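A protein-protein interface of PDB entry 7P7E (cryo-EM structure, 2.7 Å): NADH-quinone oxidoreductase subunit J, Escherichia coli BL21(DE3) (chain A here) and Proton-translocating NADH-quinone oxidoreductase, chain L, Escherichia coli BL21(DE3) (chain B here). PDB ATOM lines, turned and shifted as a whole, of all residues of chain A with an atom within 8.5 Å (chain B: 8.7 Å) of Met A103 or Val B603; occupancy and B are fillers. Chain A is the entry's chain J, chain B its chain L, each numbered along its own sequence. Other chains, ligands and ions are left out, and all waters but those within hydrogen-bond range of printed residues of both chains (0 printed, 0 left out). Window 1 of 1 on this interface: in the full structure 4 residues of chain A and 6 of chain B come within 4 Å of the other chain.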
ATOM      1  N   PRO A  96     -21.497  -3.238  34.152  1.00  0.00           N
ATOM      2  CA  PRO A  96     -20.060  -2.915  34.062  1.00  0.00           C
ATOM      3  C   PRO A  96     -19.125  -4.112  34.126  1.00  0.00           C
ATOM      4  O   PRO A  96     -18.085  -4.094  33.457  1.00  0.00           O
ATOM      5  CB  PRO A  96     -19.847  -1.980  35.257  1.00  0.00           C
ATOM      6  CG  PRO A  96     -21.151  -1.306  35.425  1.00  0.00           C
ATOM      7  CD  PRO A  96     -22.198  -2.311  35.064  1.00  0.00           C
ATOM      8  N   ALA A  97     -19.461  -5.153  34.892  1.00  0.00           N
ATOM      9  CA  ALA A  97     -18.578  -6.311  34.985  1.00  0.00           C
ATOM     10  C   ALA A  97     -18.498  -7.060  33.662  1.00  0.00           C
ATOM     11  O   ALA A  97     -17.402  -7.406  33.206  1.00  0.00           O
ATOM     12  CB  ALA A  97     -19.036  -7.246  36.102  1.00  0.00           C
ATOM     13  N   ILE A  98     -19.642  -7.305  33.016  1.00  0.00           N
ATOM     14  CA  ILE A  98     -19.588  -8.013  31.740  1.00  0.00           C
ATOM     15  C   ILE A  98     -19.031  -7.107  30.650  1.00  0.00           C
ATOM     16  O   ILE A  98     -18.408  -7.592  29.701  1.00  0.00           O
ATOM     17  CB  ILE A  98     -20.960  -8.598  31.341  1.00  0.00           C
ATOM     18  CG1 ILE A  98     -22.029  -7.510  31.218  1.00  0.00           C
ATOM     19  CG2 ILE A  98     -21.381  -9.677  32.335  1.00  0.00           C
ATOM     20  CD1 ILE A  98     -23.453  -8.036  31.161  1.00  0.00           C
ATOM     21  N   LEU A  99     -19.221  -5.790  30.771  1.00  0.00           N
ATOM     22  CA  LEU A  99     -18.617  -4.860  29.820  1.00  0.00           C
ATOM     23  C   LEU A  99     -17.094  -4.905  29.894  1.00  0.00           C
ATOM     24  O   LEU A  99     -16.404  -4.992  28.867  1.00  0.00           O
ATOM     25  CB  LEU A  99     -19.132  -3.448  30.093  1.00  0.00           C
ATOM     26  CG  LEU A  99     -18.843  -2.388  29.037  1.00  0.00           C
ATOM     27  CD1 LEU A  99     -19.704  -2.621  27.808  1.00  0.00           C
ATOM     28  CD2 LEU A  99     -19.086  -1.012  29.619  1.00  0.00           C
ATOM     29  N   SER A 100     -16.553  -4.872  31.116  1.00  0.00           N
ATOM     30  CA  SER A 100     -15.113  -4.990  31.302  1.00  0.00           C
ATOM     31  C   SER A 100     -14.607  -6.366  30.900  1.00  0.00           C
ATOM     32  O   SER A 100     -13.491  -6.482  30.387  1.00  0.00           O
ATOM     33  CB  SER A 100     -14.746  -4.691  32.753  1.00  0.00           C
ATOM     34  OG  SER A 100     -15.117  -3.369  33.103  1.00  0.00           O
ATOM     35  N   ALA A 101     -15.411  -7.412  31.106  1.00  0.00           N
ATOM     36  CA  ALA A 101     -15.020  -8.751  30.676  1.00  0.00           C
ATOM     37  C   ALA A 101     -14.951  -8.854  29.157  1.00  0.00           C
ATOM     38  O   ALA A 101     -14.050  -9.503  28.616  1.00  0.00           O
ATOM     39  CB  ALA A 101     -15.992  -9.784  31.242  1.00  0.00           C
ATOM     40  N   ILE A 102     -15.897  -8.224  28.453  1.00  0.00           N
ATOM     41  CA  ILE A 102     -15.875  -8.213  26.993  1.00  0.00           C
ATOM     42  C   ILE A 102     -14.663  -7.444  26.480  1.00  0.00           C
ATOM     43  O   ILE A 102     -13.964  -7.897  25.560  1.00  0.00           O
ATOM     44  CB  ILE A 102     -17.195  -7.634  26.451  1.00  0.00           C
ATOM     45  CG1 ILE A 102     -18.333  -8.637  26.634  1.00  0.00           C
ATOM     46  CG2 ILE A 102     -17.070  -7.255  24.984  1.00  0.00           C
ATOM     47  CD1 ILE A 102     -19.704  -8.038  26.438  1.00  0.00           C
ATOM     48  N   MET A 103     -14.385  -6.278  27.077  1.00  0.00           N
ATOM     49  CA  MET A 103     -13.201  -5.511  26.688  1.00  0.00           C
ATOM     50  C   MET A 103     -11.921  -6.301  26.948  1.00  0.00           C
ATOM     51  O   MET A 103     -11.013  -6.324  26.107  1.00  0.00           O
ATOM     52  CB  MET A 103     -13.173  -4.177  27.433  1.00  0.00           C
ATOM     53  CG  MET A 103     -11.975  -3.308  27.090  1.00  0.00           C
ATOM     54  SD  MET A 103     -11.977  -1.725  27.946  1.00  0.00           S
ATOM     55  CE  MET A 103     -13.652  -1.185  27.641  1.00  0.00           C
ATOM     56  N   LEU A 104     -11.855  -6.990  28.091  1.00  0.00           N
ATOM     57  CA  LEU A 104     -10.692  -7.802  28.423  1.00  0.00           C
ATOM     58  C   LEU A 104     -10.524  -8.965  27.455  1.00  0.00           C
ATOM     59  O   LEU A 104      -9.400  -9.282  27.057  1.00  0.00           O
ATOM     60  CB  LEU A 104     -10.810  -8.315  29.859  1.00  0.00           C
ATOM     61  CG  LEU A 104      -9.795  -9.363  30.320  1.00  0.00           C
ATOM     62  CD1 LEU A 104      -8.404  -8.764  30.395  1.00  0.00           C
ATOM     63  CD2 LEU A 104     -10.203  -9.949  31.658  1.00  0.00           C
ATOM     64  N   VAL A 105     -11.625  -9.616  27.065  1.00  0.00           N
ATOM     65  CA  VAL A 105     -11.489 -10.767  26.180  1.00  0.00           C
ATOM     66  C   VAL A 105     -11.090 -10.325  24.775  1.00  0.00           C
ATOM     67  O   VAL A 105     -10.307 -11.015  24.109  1.00  0.00           O
ATOM     68  CB  VAL A 105     -12.760 -11.650  26.203  1.00  0.00           C
ATOM     69  CG1 VAL A 105     -13.879 -11.121  25.317  1.00  0.00           C
ATOM     70  CG2 VAL A 105     -12.406 -13.077  25.814  1.00  0.00           C
ATOM     71  N   VAL A 106     -11.544  -9.149  24.325  1.00  0.00           N
ATOM     72  CA  VAL A 106     -11.087  -8.635  23.034  1.00  0.00           C
ATOM     73  C   VAL A 106      -9.605  -8.272  23.094  1.00  0.00           C
ATOM     74  O   VAL A 106      -8.831  -8.592  22.174  1.00  0.00           O
ATOM     75  CB  VAL A 106     -11.954  -7.440  22.595  1.00  0.00           C
ATOM     76  CG1 VAL A 106     -11.391  -6.807  21.339  1.00  0.00           C
ATOM     77  CG2 VAL A 106     -13.380  -7.889  22.349  1.00  0.00           C
ATOM     78  N   ILE A 107      -9.179  -7.632  24.191  1.00  0.00           N
ATOM     79  CA  ILE A 107      -7.774  -7.252  24.336  1.00  0.00           C
ATOM     80  C   ILE A 107      -6.881  -8.487  24.365  1.00  0.00           C
ATOM     81  O   ILE A 107      -5.881  -8.557  23.647  1.00  0.00           O
ATOM     82  CB  ILE A 107      -7.572  -6.374  25.585  1.00  0.00           C
ATOM     83  CG1 ILE A 107      -8.147  -4.977  25.353  1.00  0.00           C
ATOM     84  CG2 ILE A 107      -6.100  -6.258  25.926  1.00  0.00           C
ATOM     85  CD1 ILE A 107      -8.403  -4.208  26.627  1.00  0.00           C
ATOM     86  N   VAL A 108      -7.249  -9.501  25.156  1.00  0.00           N
ATOM     87  CA  VAL A 108      -6.406 -10.691  25.233  1.00  0.00           C
ATOM     88  C   VAL A 108      -6.501 -11.540  23.973  1.00  0.00           C
ATOM     89  O   VAL A 108      -5.588 -12.329  23.707  1.00  0.00           O
ATOM     90  CB  VAL A 108      -6.712 -11.548  26.479  1.00  0.00           C
ATOM     91  CG1 VAL A 108      -6.570 -10.722  27.747  1.00  0.00           C
ATOM     92  CG2 VAL A 108      -8.079 -12.201  26.385  1.00  0.00           C
ATOM     93  N   TYR A 109      -7.573 -11.410  23.185  1.00  0.00           N
ATOM     94  CA  TYR A 109      -7.555 -11.986  21.845  1.00  0.00           C
ATOM     95  C   TYR A 109      -6.498 -11.307  20.991  1.00  0.00           C
ATOM     96  O   TYR A 109      -5.798 -11.965  20.212  1.00  0.00           O
ATOM     97  CB  TYR A 109      -8.943 -11.883  21.201  1.00  0.00           C
ATOM     98  CG  TYR A 109      -8.986 -12.177  19.709  1.00  0.00           C
ATOM     99  CD1 TYR A 109      -9.232 -13.463  19.248  1.00  0.00           C
ATOM    100  CD2 TYR A 109      -8.859 -11.158  18.764  1.00  0.00           C
ATOM    101  CE1 TYR A 109      -9.285 -13.740  17.895  1.00  0.00           C
ATOM    102  CE2 TYR A 109      -8.909 -11.426  17.410  1.00  0.00           C
ATOM    103  CZ  TYR A 109      -9.127 -12.718  16.982  1.00  0.00           C
ATOM    104  OH  TYR A 109      -9.188 -12.991  15.635  1.00  0.00           O
ATOM    105  N   ALA A 110      -6.377  -9.983  21.114  1.00  0.00           N
ATOM    106  CA  ALA A 110      -5.317  -9.282  20.394  1.00  0.00           C
ATOM    107  C   ALA A 110      -3.929  -9.657  20.906  1.00  0.00           C
ATOM    108  O   ALA A 110      -2.976  -9.697  20.119  1.00  0.00           O
ATOM    109  CB  ALA A 110      -5.526  -7.775  20.484  1.00  0.00           C
ATOM    110  N   VAL B 595     -18.423   7.758  31.928  1.00  0.00           N
ATOM    111  CA  VAL B 595     -17.360   6.752  31.944  1.00  0.00           C
ATOM    112  C   VAL B 595     -17.849   5.445  31.326  1.00  0.00           C
ATOM    113  O   VAL B 595     -17.117   4.780  30.576  1.00  0.00           O
ATOM    114  CB  VAL B 595     -16.852   6.541  33.384  1.00  0.00           C
ATOM    115  CG1 VAL B 595     -15.756   5.498  33.413  1.00  0.00           C
ATOM    116  CG2 VAL B 595     -16.354   7.846  33.971  1.00  0.00           C
ATOM    117  N   ALA B 596     -19.093   5.061  31.631  1.00  0.00           N
ATOM    118  CA  ALA B 596     -19.664   3.843  31.064  1.00  0.00           C
ATOM    119  C   ALA B 596     -19.781   3.936  29.548  1.00  0.00           C
ATOM    120  O   ALA B 596     -19.506   2.965  28.840  1.00  0.00           O
ATOM    121  CB  ALA B 596     -21.028   3.562  31.692  1.00  0.00           C
ATOM    122  N   SER B 597     -20.176   5.101  29.036  1.00  0.00           N
ATOM    123  CA  SER B 597     -20.288   5.291  27.593  1.00  0.00           C
ATOM    124  C   SER B 597     -18.920   5.298  26.931  1.00  0.00           C
ATOM    125  O   SER B 597     -18.772   4.812  25.805  1.00  0.00           O
ATOM    126  CB  SER B 597     -21.042   6.585  27.291  1.00  0.00           C
ATOM    127  OG  SER B 597     -20.257   7.722  27.600  1.00  0.00           O
ATOM    128  N   MET B 598     -17.906   5.838  27.616  1.00  0.00           N
ATOM    129  CA  MET B 598     -16.541   5.747  27.102  1.00  0.00           C
ATOM    130  C   MET B 598     -16.081   4.297  27.004  1.00  0.00           C
ATOM    131  O   MET B 598     -15.469   3.899  26.006  1.00  0.00           O
ATOM    132  CB  MET B 598     -15.589   6.553  27.984  1.00  0.00           C
ATOM    133  CG  MET B 598     -15.095   7.840  27.344  1.00  0.00           C
ATOM    134  SD  MET B 598     -14.007   8.798  28.416  1.00  0.00           S
ATOM    135  CE  MET B 598     -12.586   7.716  28.517  1.00  0.00           C
ATOM    136  N   SER B 599     -16.387   3.484  28.019  1.00  0.00           N
ATOM    137  CA  SER B 599     -15.991   2.077  27.972  1.00  0.00           C
ATOM    138  C   SER B 599     -16.794   1.299  26.929  1.00  0.00           C
ATOM    139  O   SER B 599     -16.256   0.396  26.276  1.00  0.00           O
ATOM    140  CB  SER B 599     -16.133   1.440  29.354  1.00  0.00           C
ATOM    141  OG  SER B 599     -17.367   1.780  29.950  1.00  0.00           O
ATOM    142  N   ILE B 600     -18.074   1.641  26.752  1.00  0.00           N
ATOM    143  CA  ILE B 600     -18.894   1.024  25.708  1.00  0.00           C
ATOM    144  C   ILE B 600     -18.342   1.357  24.328  1.00  0.00           C
ATOM    145  O   ILE B 600     -18.243   0.485  23.454  1.00  0.00           O
ATOM    146  CB  ILE B 600     -20.364   1.465  25.854  1.00  0.00           C
ATOM    147  CG1 ILE B 600     -21.035   0.750  27.023  1.00  0.00           C
ATOM    148  CG2 ILE B 600     -21.155   1.194  24.583  1.00  0.00           C
ATOM    149  CD1 ILE B 600     -22.280   1.443  27.522  1.00  0.00           C
ATOM    150  N   GLY B 601     -17.965   2.619  24.113  1.00  0.00           N
ATOM    151  CA  GLY B 601     -17.359   2.999  22.848  1.00  0.00           C
ATOM    152  C   GLY B 601     -16.016   2.337  22.619  1.00  0.00           C
ATOM    153  O   GLY B 601     -15.670   1.996  21.486  1.00  0.00           O
ATOM    154  N   ALA B 602     -15.244   2.142  23.691  1.00  0.00           N
ATOM    155  CA  ALA B 602     -14.000   1.388  23.579  1.00  0.00           C
ATOM    156  C   ALA B 602     -14.265  -0.050  23.160  1.00  0.00           C
ATOM    157  O   ALA B 602     -13.553  -0.594  22.305  1.00  0.00           O
ATOM    158  CB  ALA B 602     -13.240   1.430  24.903  1.00  0.00           C
ATOM    159  N   VAL B 603     -15.294  -0.671  23.742  1.00  0.00           N
ATOM    160  CA  VAL B 603     -15.675  -2.035  23.379  1.00  0.00           C
ATOM    161  C   VAL B 603     -16.081  -2.105  21.911  1.00  0.00           C
ATOM    162  O   VAL B 603     -15.653  -3.002  21.173  1.00  0.00           O
ATOM    163  CB  VAL B 603     -16.800  -2.531  24.310  1.00  0.00           C
ATOM    164  CG1 VAL B 603     -17.631  -3.623  23.654  1.00  0.00           C
ATOM    165  CG2 VAL B 603     -16.223  -3.024  25.621  1.00  0.00           C
ATOM    166  N   VAL B 604     -16.886  -1.139  21.461  1.00  0.00           N
ATOM    167  CA  VAL B 604     -17.365  -1.121  20.081  1.00  0.00           C
ATOM    168  C   VAL B 604     -16.208  -0.920  19.106  1.00  0.00           C
ATOM    169  O   VAL B 604     -16.115  -1.617  18.088  1.00  0.00           O
ATOM    170  CB  VAL B 604     -18.449  -0.039  19.917  1.00  0.00           C
ATOM    171  CG1 VAL B 604     -18.739   0.231  18.447  1.00  0.00           C
ATOM    172  CG2 VAL B 604     -19.718  -0.456  20.637  1.00  0.00           C
ATOM    173  N   VAL B 605     -15.299   0.012  19.412  1.00  0.00           N
ATOM    174  CA  VAL B 605     -14.159   0.281  18.538  1.00  0.00           C
ATOM    175  C   VAL B 605     -13.239  -0.934  18.458  1.00  0.00           C
ATOM    176  O   VAL B 605     -12.801  -1.326  17.368  1.00  0.00           O
ATOM    177  CB  VAL B 605     -13.409   1.540  19.022  1.00  0.00           C
ATOM    178  CG1 VAL B 605     -12.002   1.601  18.453  1.00  0.00           C
ATOM    179  CG2 VAL B 605     -14.182   2.790  18.643  1.00  0.00           C
ATOM    180  N   LEU B 606     -12.955  -1.564  19.604  1.00  0.00           N
ATOM    181  CA  LEU B 606     -12.090  -2.740  19.616  1.00  0.00           C
ATOM    182  C   LEU B 606     -12.720  -3.910  18.865  1.00  0.00           C
ATOM    183  O   LEU B 606     -12.033  -4.608  18.109  1.00  0.00           O
ATOM    184  CB  LEU B 606     -11.774  -3.136  21.056  1.00  0.00           C
ATOM    185  CG  LEU B 606     -10.736  -2.287  21.789  1.00  0.00           C
ATOM    186  CD1 LEU B 606     -10.839  -2.504  23.288  1.00  0.00           C
ATOM    187  CD2 LEU B 606      -9.341  -2.610  21.295  1.00  0.00           C
ATOM    188  N   ALA B 607     -14.028  -4.126  19.044  1.00  0.00           N
ATOM    189  CA  ALA B 607     -14.709  -5.207  18.338  1.00  0.00           C
ATOM    190  C   ALA B 607     -14.749  -4.959  16.836  1.00  0.00           C
ATOM    191  O   ALA B 607     -14.542  -5.886  16.044  1.00  0.00           O
ATOM    192  CB  ALA B 607     -16.123  -5.381  18.891  1.00  0.00           C
ATOM    193  N   LEU B 608     -15.007  -3.712  16.424  1.00  0.00           N
ATOM    194  CA  LEU B 608     -15.021  -3.382  15.003  1.00  0.00           C
ATOM    195  C   LEU B 608     -13.643  -3.547  14.380  1.00  0.00           C
ATOM    196  O   LEU B 608     -13.524  -4.019  13.247  1.00  0.00           O
ATOM    197  CB  LEU B 608     -15.531  -1.957  14.800  1.00  0.00           C
ATOM    198  CG  LEU B 608     -17.041  -1.737  14.881  1.00  0.00           C
ATOM    199  CD1 LEU B 608     -17.356  -0.254  14.920  1.00  0.00           C
ATOM    200  CD2 LEU B 608     -17.747  -2.408  13.718  1.00  0.00           C
ATOM    201  N   LEU B 609     -12.590  -3.169  15.107  1.00  0.00           N
ATOM    202  CA  LEU B 609     -11.243  -3.336  14.577  1.00  0.00           C
ATOM    203  C   LEU B 609     -10.837  -4.801  14.513  1.00  0.00           C
ATOM    204  O   LEU B 609     -10.095  -5.195  13.607  1.00  0.00           O
ATOM    205  CB  LEU B 609     -10.248  -2.542  15.417  1.00  0.00           C
ATOM    206  CG  LEU B 609     -10.177  -1.059  15.067  1.00  0.00           C
ATOM    207  CD1 LEU B 609      -9.313  -0.337  16.059  1.00  0.00           C
ATOM    208  CD2 LEU B 609      -9.641  -0.869  13.666  1.00  0.00           C
ATOM    209  N   MET B 610     -11.304  -5.622  15.457  1.00  0.00           N
ATOM    210  CA  MET B 610     -10.986  -7.044  15.403  1.00  0.00           C
ATOM    211  C   MET B 610     -11.786  -7.776  14.334  1.00  0.00           C
ATOM    212  O   MET B 610     -11.313  -8.788  13.805  1.00  0.00           O
ATOM    213  CB  MET B 610     -11.217  -7.691  16.769  1.00  0.00           C
ATOM    214  CG  MET B 610     -10.183  -7.340  17.841  1.00  0.00           C
ATOM    215  SD  MET B 610      -8.452  -7.389  17.319  1.00  0.00           S
ATOM    216  CE  MET B 610      -8.078  -5.648  17.091  1.00  0.00           C
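O of Val B595 sits at hydrogen-bond distance from OG of Ser B599, 3.1 Å away.
The backbone carbonyl oxygen (O) of Ala B596 is in hydrogen-bond range of the side-chain hydroxyl (OG) of Ser B599 (2.7 Å).
No residue of chain A comes within 4 Å of Gly B601.
Printed residues of chain A within 4 Å of Leu B606: Val A106.
Of the printed residues of chain A, Ile B600 touches Leu A99 (3.7 Å).
The nearest residue of chain B that does not touch Met A103 is Leu B606 (4.05 Å).
The nearest residue of chain A that does not touch Val B603 is Val A106 (5.5 Å).
Of the 15 printed residues of chain A, 4 touch a printed residue of chain B.
Hydrophobic or aromatic side chains of chain A that line the printed part of chain B: Leu A99, Ile A102, Met A103 and Val A106.
Of the 16 printed residues of chain B, 6 touch a printed residue of chain A.
Printed residues of chain B that touch a printed residue of chain A: Ser B599, Ile B600, Ala B602, Val B603, Leu B606 and Met B610.
Hydrophobic or aromatic side chains of chain B within 4 Å of the printed part of chain A: Ile B600, Ala B602, Val B603, Leu B606 and Met B610.
Among the printed residues, 9 pairs touch across the chains.
Leu A99 touches Ser B599.
Leu A99 touches Ile B600 (CD2 to CG1, 3.7 Å).
Leu A99 touches Val B603.
CG1 of Val B603 touches CG2 of Ile A102, at 3.9 Å.
Ser B599 touches Met A103 (O to CE, 3.3 Å).
Met A103 touches Ala B602 (CE to CB, 3.8 Å).
Val B603 touches Met A103.
CG1 of Val A106 touches CB of Leu B606, at 3.7 Å.
Val A106 touches Met B610.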
